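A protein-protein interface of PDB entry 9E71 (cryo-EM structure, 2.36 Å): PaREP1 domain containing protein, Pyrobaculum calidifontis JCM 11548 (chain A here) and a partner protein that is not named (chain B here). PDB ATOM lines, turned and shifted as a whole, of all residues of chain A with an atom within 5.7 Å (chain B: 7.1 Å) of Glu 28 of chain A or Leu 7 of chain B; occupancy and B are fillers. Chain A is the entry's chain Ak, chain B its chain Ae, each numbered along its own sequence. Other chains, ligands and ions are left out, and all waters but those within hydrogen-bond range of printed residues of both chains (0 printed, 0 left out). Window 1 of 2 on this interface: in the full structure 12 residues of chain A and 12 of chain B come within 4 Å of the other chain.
Of the 12 printed residues of chain B, 7 touch a printed residue of chain A. Hydrophobic or aromatic side chains of chain B that line the printed part of chain A: Ile 5, Phe 6, Leu 7, Val 8 and Leu 10. Along chain A the printed residues that touch a printed residue of chain B span positions 24 to 68.
Ala 23 of chain A touches none of the printed residues of chain B. Glu 28 of chain A touches five residues of chain B. Of the printed residues of chain A, Phe 6 of chain B touches Glu 28 (2.7 Å), Val 31 (3.6 Å), Glu 32 (3.5 Å) and Glu 68 (3.0 Å). Of the printed residues of chain A, Leu 7 of chain B touches Leu 24 (3.8 Å), Arg 27 (3.9 Å), Glu 28 (3.0 Å) and Glu 68 (3.1 Å). Printed residues of chain A within 4 Å of Val 8 of chain B: Glu 68. Printed residues of chain A within 4 Å of Leu 10 of chain B: Leu 24, Glu 25 and Glu 28. The nearest residue of chain B that does not touch Glu 28 of chain A is Val 8 of chain B (6.1 Å).
The side-chain carboxylate of Glu 28 of chain A is in hydrogen-bond range of the backbone NH of Phe 6 of chain B, 2.7 Å away. The backbone NH (N) of Leu 7 of chain B lies within hydrogen-bond range of the side-chain carboxylate (OE1) of Glu 28 of chain A. The side-chain carboxylate (OE2) of Glu 68 of chain A lies within hydrogen-bond range of the backbone NH (N) of Val 8 of chain B, at 2.8 Å.
OE2 of Glu 28 of chain A lies close to OE2 of Glu 32 of chain A, 2.7 Å away. The backbone carbonyl oxygen (O) of Thr 42 of chain B is in hydrogen-bond range of the backbone NH (N) of Ile 5 of chain B, at 2.9 Å.
CD1 of Leu 7 of chain B touches CD1 of Leu 24 of chain A (3.8 Å). Glu 9 of chain B touches Leu 24 of chain A (OE1 to CD1, 3.9 Å). CD1 of Leu 10 of chain B touches CD2 of Leu 24 of chain A (3.9 Å). Glu 25 of chain A touches Leu 10 of chain B. Glu 4 of chain B touches Glu 28 of chain A. CA of Ile 5 of chain B touches OE2 of Glu 28 of chain A (3.3 Å). Leu 10 of chain B touches Glu 28 of chain A. Glu 32 of chain A touches Glu 4 of chain B. CD2 of Phe 6 of chain B touches CG of Glu 32 of chain A, at 3.5 Å. Phe 6 of chain B touches Glu 68 of chain A.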
ATOM      1  N   ALA A  23     -25.499 -30.568   1.695  1.00  0.00           N
ATOM      2  CA  ALA A  23     -24.060 -30.801   1.681  1.00  0.00           C
ATOM      3  C   ALA A  23     -23.294 -29.486   1.617  1.00  0.00           C
ATOM      4  O   ALA A  23     -22.275 -29.317   2.295  1.00  0.00           O
ATOM      5  CB  ALA A  23     -23.687 -31.703   0.507  1.00  0.00           C
ATOM      6  N   LEU A  24     -23.778 -28.543   0.809  1.00  0.00           N
ATOM      7  CA  LEU A  24     -23.171 -27.217   0.761  1.00  0.00           C
ATOM      8  C   LEU A  24     -23.296 -26.501   2.100  1.00  0.00           C
ATOM      9  O   LEU A  24     -22.338 -25.873   2.571  1.00  0.00           O
ATOM     10  CB  LEU A  24     -23.817 -26.392  -0.350  1.00  0.00           C
ATOM     11  CG  LEU A  24     -23.229 -25.007  -0.614  1.00  0.00           C
ATOM     12  CD1 LEU A  24     -21.734 -25.094  -0.833  1.00  0.00           C
ATOM     13  CD2 LEU A  24     -23.912 -24.358  -1.797  1.00  0.00           C
ATOM     14  N   GLU A  25     -24.474 -26.586   2.729  1.00  0.00           N
ATOM     15  CA  GLU A  25     -24.663 -25.968   4.041  1.00  0.00           C
ATOM     16  C   GLU A  25     -23.743 -26.585   5.087  1.00  0.00           C
ATOM     17  O   GLU A  25     -23.194 -25.879   5.936  1.00  0.00           O
ATOM     18  CB  GLU A  25     -26.119 -26.094   4.489  1.00  0.00           C
ATOM     19  CG  GLU A  25     -27.144 -25.635   3.472  1.00  0.00           C
ATOM     20  CD  GLU A  25     -26.961 -24.193   3.062  1.00  0.00           C
ATOM     21  OE1 GLU A  25     -27.494 -23.303   3.755  1.00  0.00           O
ATOM     22  OE2 GLU A  25     -26.282 -23.954   2.044  1.00  0.00           O
ATOM     23  N   PHE A  26     -23.553 -27.902   5.033  1.00  0.00           N
ATOM     24  CA  PHE A  26     -22.691 -28.567   6.000  1.00  0.00           C
ATOM     25  C   PHE A  26     -21.226 -28.229   5.763  1.00  0.00           C
ATOM     26  O   PHE A  26     -20.450 -28.118   6.718  1.00  0.00           O
ATOM     27  CB  PHE A  26     -22.916 -30.075   5.947  1.00  0.00           C
ATOM     28  CG  PHE A  26     -24.238 -30.508   6.508  1.00  0.00           C
ATOM     29  CD1 PHE A  26     -24.793 -29.846   7.586  1.00  0.00           C
ATOM     30  CD2 PHE A  26     -24.922 -31.577   5.959  1.00  0.00           C
ATOM     31  CE1 PHE A  26     -26.007 -30.241   8.103  1.00  0.00           C
ATOM     32  CE2 PHE A  26     -26.136 -31.976   6.471  1.00  0.00           C
ATOM     33  CZ  PHE A  26     -26.678 -31.309   7.545  1.00  0.00           C
ATOM     34  N   ARG A  27     -20.825 -28.071   4.499  1.00  0.00           N
ATOM     35  CA  ARG A  27     -19.471 -27.611   4.207  1.00  0.00           C
ATOM     36  C   ARG A  27     -19.240 -26.213   4.761  1.00  0.00           C
ATOM     37  O   ARG A  27     -18.186 -25.929   5.351  1.00  0.00           O
ATOM     38  CB  ARG A  27     -19.225 -27.629   2.701  1.00  0.00           C
ATOM     39  CG  ARG A  27     -18.348 -28.760   2.227  1.00  0.00           C
ATOM     40  CD  ARG A  27     -17.774 -28.458   0.855  1.00  0.00           C
ATOM     41  NE  ARG A  27     -17.334 -29.665   0.165  1.00  0.00           N
ATOM     42  CZ  ARG A  27     -18.140 -30.625  -0.264  1.00  0.00           C
ATOM     43  NH1 ARG A  27     -19.452 -30.547  -0.114  1.00  0.00           N
ATOM     44  NH2 ARG A  27     -17.618 -31.691  -0.859  1.00  0.00           N
ATOM     45  N   GLU A  28     -20.230 -25.333   4.589  1.00  0.00           N
ATOM     46  CA  GLU A  28     -20.146 -23.995   5.160  1.00  0.00           C
ATOM     47  C   GLU A  28     -20.056 -24.044   6.682  1.00  0.00           C
ATOM     48  O   GLU A  28     -19.273 -23.306   7.287  1.00  0.00           O
ATOM     49  CB  GLU A  28     -21.350 -23.171   4.716  1.00  0.00           C
ATOM     50  CG  GLU A  28     -21.508 -21.864   5.448  1.00  0.00           C
ATOM     51  CD  GLU A  28     -20.555 -20.808   4.941  1.00  0.00           C
ATOM     52  OE1 GLU A  28     -19.891 -21.051   3.915  1.00  0.00           O
ATOM     53  OE2 GLU A  28     -20.466 -19.734   5.567  1.00  0.00           O
ATOM     54  N   LYS A  29     -20.840 -24.920   7.315  1.00  0.00           N
ATOM     55  CA  LYS A  29     -20.805 -25.039   8.769  1.00  0.00           C
ATOM     56  C   LYS A  29     -19.460 -25.560   9.257  1.00  0.00           C
ATOM     57  O   LYS A  29     -18.956 -25.112  10.291  1.00  0.00           O
ATOM     58  CB  LYS A  29     -21.930 -25.951   9.253  1.00  0.00           C
ATOM     59  CG  LYS A  29     -23.314 -25.424   8.967  1.00  0.00           C
ATOM     60  CD  LYS A  29     -23.963 -24.881  10.214  1.00  0.00           C
ATOM     61  CE  LYS A  29     -25.353 -24.352   9.920  1.00  0.00           C
ATOM     62  NZ  LYS A  29     -25.478 -22.913  10.272  1.00  0.00           N
ATOM     63  N   LEU A  30     -18.871 -26.517   8.537  1.00  0.00           N
ATOM     64  CA  LEU A  30     -17.563 -27.036   8.924  1.00  0.00           C
ATOM     65  C   LEU A  30     -16.485 -25.966   8.810  1.00  0.00           C
ATOM     66  O   LEU A  30     -15.623 -25.836   9.695  1.00  0.00           O
ATOM     67  CB  LEU A  30     -17.213 -28.251   8.067  1.00  0.00           C
ATOM     68  CG  LEU A  30     -15.734 -28.556   7.834  1.00  0.00           C
ATOM     69  CD1 LEU A  30     -15.066 -29.002   9.118  1.00  0.00           C
ATOM     70  CD2 LEU A  30     -15.583 -29.613   6.765  1.00  0.00           C
ATOM     71  N   VAL A  31     -16.523 -25.182   7.729  1.00  0.00           N
ATOM     72  CA  VAL A  31     -15.568 -24.089   7.577  1.00  0.00           C
ATOM     73  C   VAL A  31     -15.762 -23.054   8.676  1.00  0.00           C
ATOM     74  O   VAL A  31     -14.789 -22.519   9.221  1.00  0.00           O
ATOM     75  CB  VAL A  31     -15.690 -23.453   6.184  1.00  0.00           C
ATOM     76  CG1 VAL A  31     -14.968 -22.126   6.162  1.00  0.00           C
ATOM     77  CG2 VAL A  31     -15.124 -24.382   5.136  1.00  0.00           C
ATOM     78  N   GLU A  32     -17.018 -22.758   9.015  1.00  0.00           N
ATOM     79  CA  GLU A  32     -17.308 -21.822  10.096  1.00  0.00           C
ATOM     80  C   GLU A  32     -16.766 -22.331  11.423  1.00  0.00           C
ATOM     81  O   GLU A  32     -16.176 -21.567  12.192  1.00  0.00           O
ATOM     82  CB  GLU A  32     -18.814 -21.585  10.191  1.00  0.00           C
ATOM     83  CG  GLU A  32     -19.329 -20.491   9.292  1.00  0.00           C
ATOM     84  CD  GLU A  32     -20.809 -20.628   9.014  1.00  0.00           C
ATOM     85  OE1 GLU A  32     -21.460 -21.467   9.664  1.00  0.00           O
ATOM     86  OE2 GLU A  32     -21.326 -19.886   8.154  1.00  0.00           O
ATOM     87  N   CYS A  33     -16.945 -23.627  11.690  1.00  0.00           N
ATOM     88  CA  CYS A  33     -16.448 -24.259  12.908  1.00  0.00           C
ATOM     89  C   CYS A  33     -14.943 -24.079  13.046  1.00  0.00           C
ATOM     90  O   CYS A  33     -14.455 -23.517  14.039  1.00  0.00           O
ATOM     91  CB  CYS A  33     -16.823 -25.746  12.884  1.00  0.00           C
ATOM     92  SG  CYS A  33     -16.047 -26.809  14.115  1.00  0.00           S
ATOM     93  N   ILE A  66     -11.633 -27.369  -0.319  1.00  0.00           N
ATOM     94  CA  ILE A  66     -12.157 -26.061   0.065  1.00  0.00           C
ATOM     95  C   ILE A  66     -11.016 -25.054   0.012  1.00  0.00           C
ATOM     96  O   ILE A  66     -10.059 -25.147   0.791  1.00  0.00           O
ATOM     97  CB  ILE A  66     -12.797 -26.092   1.455  1.00  0.00           C
ATOM     98  CG1 ILE A  66     -14.022 -27.000   1.440  1.00  0.00           C
ATOM     99  CG2 ILE A  66     -13.177 -24.689   1.891  1.00  0.00           C
ATOM    100  CD1 ILE A  66     -14.294 -27.658   2.763  1.00  0.00           C
ATOM    101  N   GLU A  68     -11.428 -21.668   0.443  1.00  0.00           N
ATOM    102  CA  GLU A  68     -11.627 -20.623   1.438  1.00  0.00           C
ATOM    103  C   GLU A  68     -10.983 -20.998   2.763  1.00  0.00           C
ATOM    104  O   GLU A  68     -10.460 -20.132   3.475  1.00  0.00           O
ATOM    105  CB  GLU A  68     -13.119 -20.359   1.619  1.00  0.00           C
ATOM    106  CG  GLU A  68     -13.799 -19.838   0.376  1.00  0.00           C
ATOM    107  CD  GLU A  68     -14.440 -20.940  -0.446  1.00  0.00           C
ATOM    108  OE1 GLU A  68     -13.947 -22.086  -0.412  1.00  0.00           O
ATOM    109  OE2 GLU A  68     -15.452 -20.660  -1.118  1.00  0.00           O
ATOM    110  N   GLU B   4     -22.711 -13.934   7.947  1.00  0.00           N
ATOM    111  CA  GLU B   4     -21.423 -14.118   7.302  1.00  0.00           C
ATOM    112  C   GLU B   4     -21.401 -15.455   6.580  1.00  0.00           C
ATOM    113  O   GLU B   4     -21.831 -16.471   7.132  1.00  0.00           O
ATOM    114  CB  GLU B   4     -20.286 -14.043   8.318  1.00  0.00           C
ATOM    115  CG  GLU B   4     -18.914 -14.257   7.720  1.00  0.00           C
ATOM    116  CD  GLU B   4     -17.810 -14.078   8.734  1.00  0.00           C
ATOM    117  OE1 GLU B   4     -18.118 -14.033   9.940  1.00  0.00           O
ATOM    118  OE2 GLU B   4     -16.636 -13.978   8.327  1.00  0.00           O
ATOM    119  N   ILE B   5     -20.909 -15.445   5.349  1.00  0.00           N
ATOM    120  CA  ILE B   5     -20.734 -16.651   4.554  1.00  0.00           C
ATOM    121  C   ILE B   5     -19.251 -16.816   4.267  1.00  0.00           C
ATOM    122  O   ILE B   5     -18.506 -15.838   4.169  1.00  0.00           O
ATOM    123  CB  ILE B   5     -21.551 -16.581   3.249  1.00  0.00           C
ATOM    124  CG1 ILE B   5     -23.006 -16.253   3.564  1.00  0.00           C
ATOM    125  CG2 ILE B   5     -21.473 -17.886   2.479  1.00  0.00           C
ATOM    126  CD1 ILE B   5     -23.902 -16.315   2.365  1.00  0.00           C
ATOM    127  N   PHE B   6     -18.815 -18.067   4.156  1.00  0.00           N
ATOM    128  CA  PHE B   6     -17.420 -18.354   3.858  1.00  0.00           C
ATOM    129  C   PHE B   6     -17.194 -18.907   2.462  1.00  0.00           C
ATOM    130  O   PHE B   6     -16.146 -18.640   1.876  1.00  0.00           O
ATOM    131  CB  PHE B   6     -16.847 -19.341   4.879  1.00  0.00           C
ATOM    132  CG  PHE B   6     -16.391 -18.695   6.149  1.00  0.00           C
ATOM    133  CD1 PHE B   6     -15.128 -18.149   6.248  1.00  0.00           C
ATOM    134  CD2 PHE B   6     -17.226 -18.636   7.250  1.00  0.00           C
ATOM    135  CE1 PHE B   6     -14.706 -17.556   7.420  1.00  0.00           C
ATOM    136  CE2 PHE B   6     -16.809 -18.045   8.420  1.00  0.00           C
ATOM    137  CZ  PHE B   6     -15.547 -17.504   8.504  1.00  0.00           C
ATOM    138  N   LEU B   7     -18.142 -19.657   1.914  1.00  0.00           N
ATOM    139  CA  LEU B   7     -17.979 -20.268   0.604  1.00  0.00           C
ATOM    140  C   LEU B   7     -18.549 -19.356  -0.472  1.00  0.00           C
ATOM    141  O   LEU B   7     -19.683 -18.882  -0.357  1.00  0.00           O
ATOM    142  CB  LEU B   7     -18.658 -21.636   0.558  1.00  0.00           C
ATOM    143  CG  LEU B   7     -18.301 -22.584   1.698  1.00  0.00           C
ATOM    144  CD1 LEU B   7     -18.951 -23.936   1.491  1.00  0.00           C
ATOM    145  CD2 LEU B   7     -16.796 -22.723   1.834  1.00  0.00           C
ATOM    146  N   VAL B   8     -17.755 -19.116  -1.516  1.00  0.00           N
ATOM    147  CA  VAL B   8     -18.166 -18.211  -2.586  1.00  0.00           C
ATOM    148  C   VAL B   8     -19.367 -18.771  -3.332  1.00  0.00           C
ATOM    149  O   VAL B   8     -20.244 -18.021  -3.775  1.00  0.00           O
ATOM    150  CB  VAL B   8     -16.988 -17.942  -3.537  1.00  0.00           C
ATOM    151  CG1 VAL B   8     -17.472 -17.216  -4.777  1.00  0.00           C
ATOM    152  CG2 VAL B   8     -15.909 -17.148  -2.828  1.00  0.00           C
ATOM    153  N   GLU B   9     -19.421 -20.095  -3.489  1.00  0.00           N
ATOM    154  CA  GLU B   9     -20.544 -20.728  -4.173  1.00  0.00           C
ATOM    155  C   GLU B   9     -21.847 -20.503  -3.418  1.00  0.00           C
ATOM    156  O   GLU B   9     -22.886 -20.213  -4.022  1.00  0.00           O
ATOM    157  CB  GLU B   9     -20.275 -22.222  -4.338  1.00  0.00           C
ATOM    158  CG  GLU B   9     -21.515 -23.035  -4.636  1.00  0.00           C
ATOM    159  CD  GLU B   9     -21.222 -24.512  -4.780  1.00  0.00           C
ATOM    160  OE1 GLU B   9     -20.136 -24.951  -4.345  1.00  0.00           O
ATOM    161  OE2 GLU B   9     -22.082 -25.238  -5.322  1.00  0.00           O
ATOM    162  N   LEU B  10     -21.812 -20.637  -2.093  1.00  0.00           N
ATOM    163  CA  LEU B  10     -22.994 -20.340  -1.295  1.00  0.00           C
ATOM    164  C   LEU B  10     -23.324 -18.854  -1.333  1.00  0.00           C
ATOM    165  O   LEU B  10     -24.492 -18.472  -1.456  1.00  0.00           O
ATOM    166  CB  LEU B  10     -22.785 -20.813   0.142  1.00  0.00           C
ATOM    167  CG  LEU B  10     -23.985 -20.691   1.082  1.00  0.00           C
ATOM    168  CD1 LEU B  10     -25.166 -21.492   0.572  1.00  0.00           C
ATOM    169  CD2 LEU B  10     -23.600 -21.127   2.484  1.00  0.00           C
ATOM    170  N   TRP B  11     -22.301 -17.998  -1.243  1.00  0.00           N
ATOM    171  CA  TRP B  11     -22.544 -16.560  -1.164  1.00  0.00           C
ATOM    172  C   TRP B  11     -23.112 -16.006  -2.461  1.00  0.00           C
ATOM    173  O   TRP B  11     -23.838 -15.008  -2.436  1.00  0.00           O
ATOM    174  CB  TRP B  11     -21.256 -15.819  -0.804  1.00  0.00           C
ATOM    175  CG  TRP B  11     -21.448 -14.339  -0.644  1.00  0.00           C
ATOM    176  CD1 TRP B  11     -21.822 -13.681   0.490  1.00  0.00           C
ATOM    177  CD2 TRP B  11     -21.284 -13.338  -1.652  1.00  0.00           C
ATOM    178  NE1 TRP B  11     -21.901 -12.334   0.250  1.00  0.00           N
ATOM    179  CE2 TRP B  11     -21.577 -12.096  -1.058  1.00  0.00           C
ATOM    180  CE3 TRP B  11     -20.924 -13.371  -3.000  1.00  0.00           C
ATOM    181  CZ2 TRP B  11     -21.515 -10.901  -1.764  1.00  0.00           C
ATOM    182  CZ3 TRP B  11     -20.863 -12.187  -3.698  1.00  0.00           C
ATOM    183  CH2 TRP B  11     -21.156 -10.968  -3.080  1.00  0.00           C
ATOM    184  N   LYS B  12     -22.776 -16.616  -3.598  1.00  0.00           N
ATOM    185  CA  LYS B  12     -23.241 -16.091  -4.875  1.00  0.00           C
ATOM    186  C   LYS B  12     -24.750 -16.217  -5.021  1.00  0.00           C
ATOM    187  O   LYS B  12     -25.373 -15.387  -5.690  1.00  0.00           O
ATOM    188  CB  LYS B  12     -22.531 -16.804  -6.021  1.00  0.00           C
ATOM    189  CG  LYS B  12     -21.194 -16.193  -6.378  1.00  0.00           C
ATOM    190  CD  LYS B  12     -20.836 -16.452  -7.824  1.00  0.00           C
ATOM    191  CE  LYS B  12     -19.905 -17.636  -7.954  1.00  0.00           C
ATOM    192  NZ  LYS B  12     -18.957 -17.473  -9.084  1.00  0.00           N
ATOM    193  N   THR B  42     -22.192 -11.014   4.278  1.00  0.00           N
ATOM    194  CA  THR B  42     -20.817 -10.573   4.105  1.00  0.00           C
ATOM    195  C   THR B  42     -19.902 -11.772   3.907  1.00  0.00           C
ATOM    196  O   THR B  42     -20.026 -12.781   4.606  1.00  0.00           O
ATOM    197  CB  THR B  42     -20.345  -9.757   5.311  1.00  0.00           C
ATOM    198  OG1 THR B  42     -21.058  -8.517   5.356  1.00  0.00           O
ATOM    199  CG2 THR B  42     -18.855  -9.471   5.220  1.00  0.00           C
ATOM    200  N   ILE B  43     -18.995 -11.661   2.944  1.00  0.00           N
ATOM    201  CA  ILE B  43     -17.954 -12.660   2.739  1.00  0.00           C
ATOM    202  C   ILE B  43     -16.619 -11.954   2.559  1.00  0.00           C
ATOM    203  O   ILE B  43     -16.526 -10.949   1.848  1.00  0.00           O
ATOM    204  CB  ILE B  43     -18.255 -13.568   1.533  1.00  0.00           C
ATOM    205  CG1 ILE B  43     -17.166 -14.629   1.397  1.00  0.00           C
ATOM    206  CG2 ILE B  43     -18.367 -12.749   0.263  1.00  0.00           C
ATOM    207  CD1 ILE B  43     -17.648 -15.915   0.802  1.00  0.00           C
ATOM    208  N   VAL B  45     -12.987 -12.294   0.983  1.00  0.00           N
ATOM    209  CA  VAL B  45     -12.366 -13.063  -0.094  1.00  0.00           C
ATOM    210  C   VAL B  45     -10.993 -12.477  -0.385  1.00  0.00           C
ATOM    211  O   VAL B  45     -10.681 -11.350   0.026  1.00  0.00           O
ATOM    212  CB  VAL B  45     -13.242 -13.072  -1.368  1.00  0.00           C
ATOM    213  CG1 VAL B  45     -14.607 -13.648  -1.063  1.00  0.00           C
ATOM    214  CG2 VAL B  45     -13.369 -11.673  -1.936  1.00  0.00           C
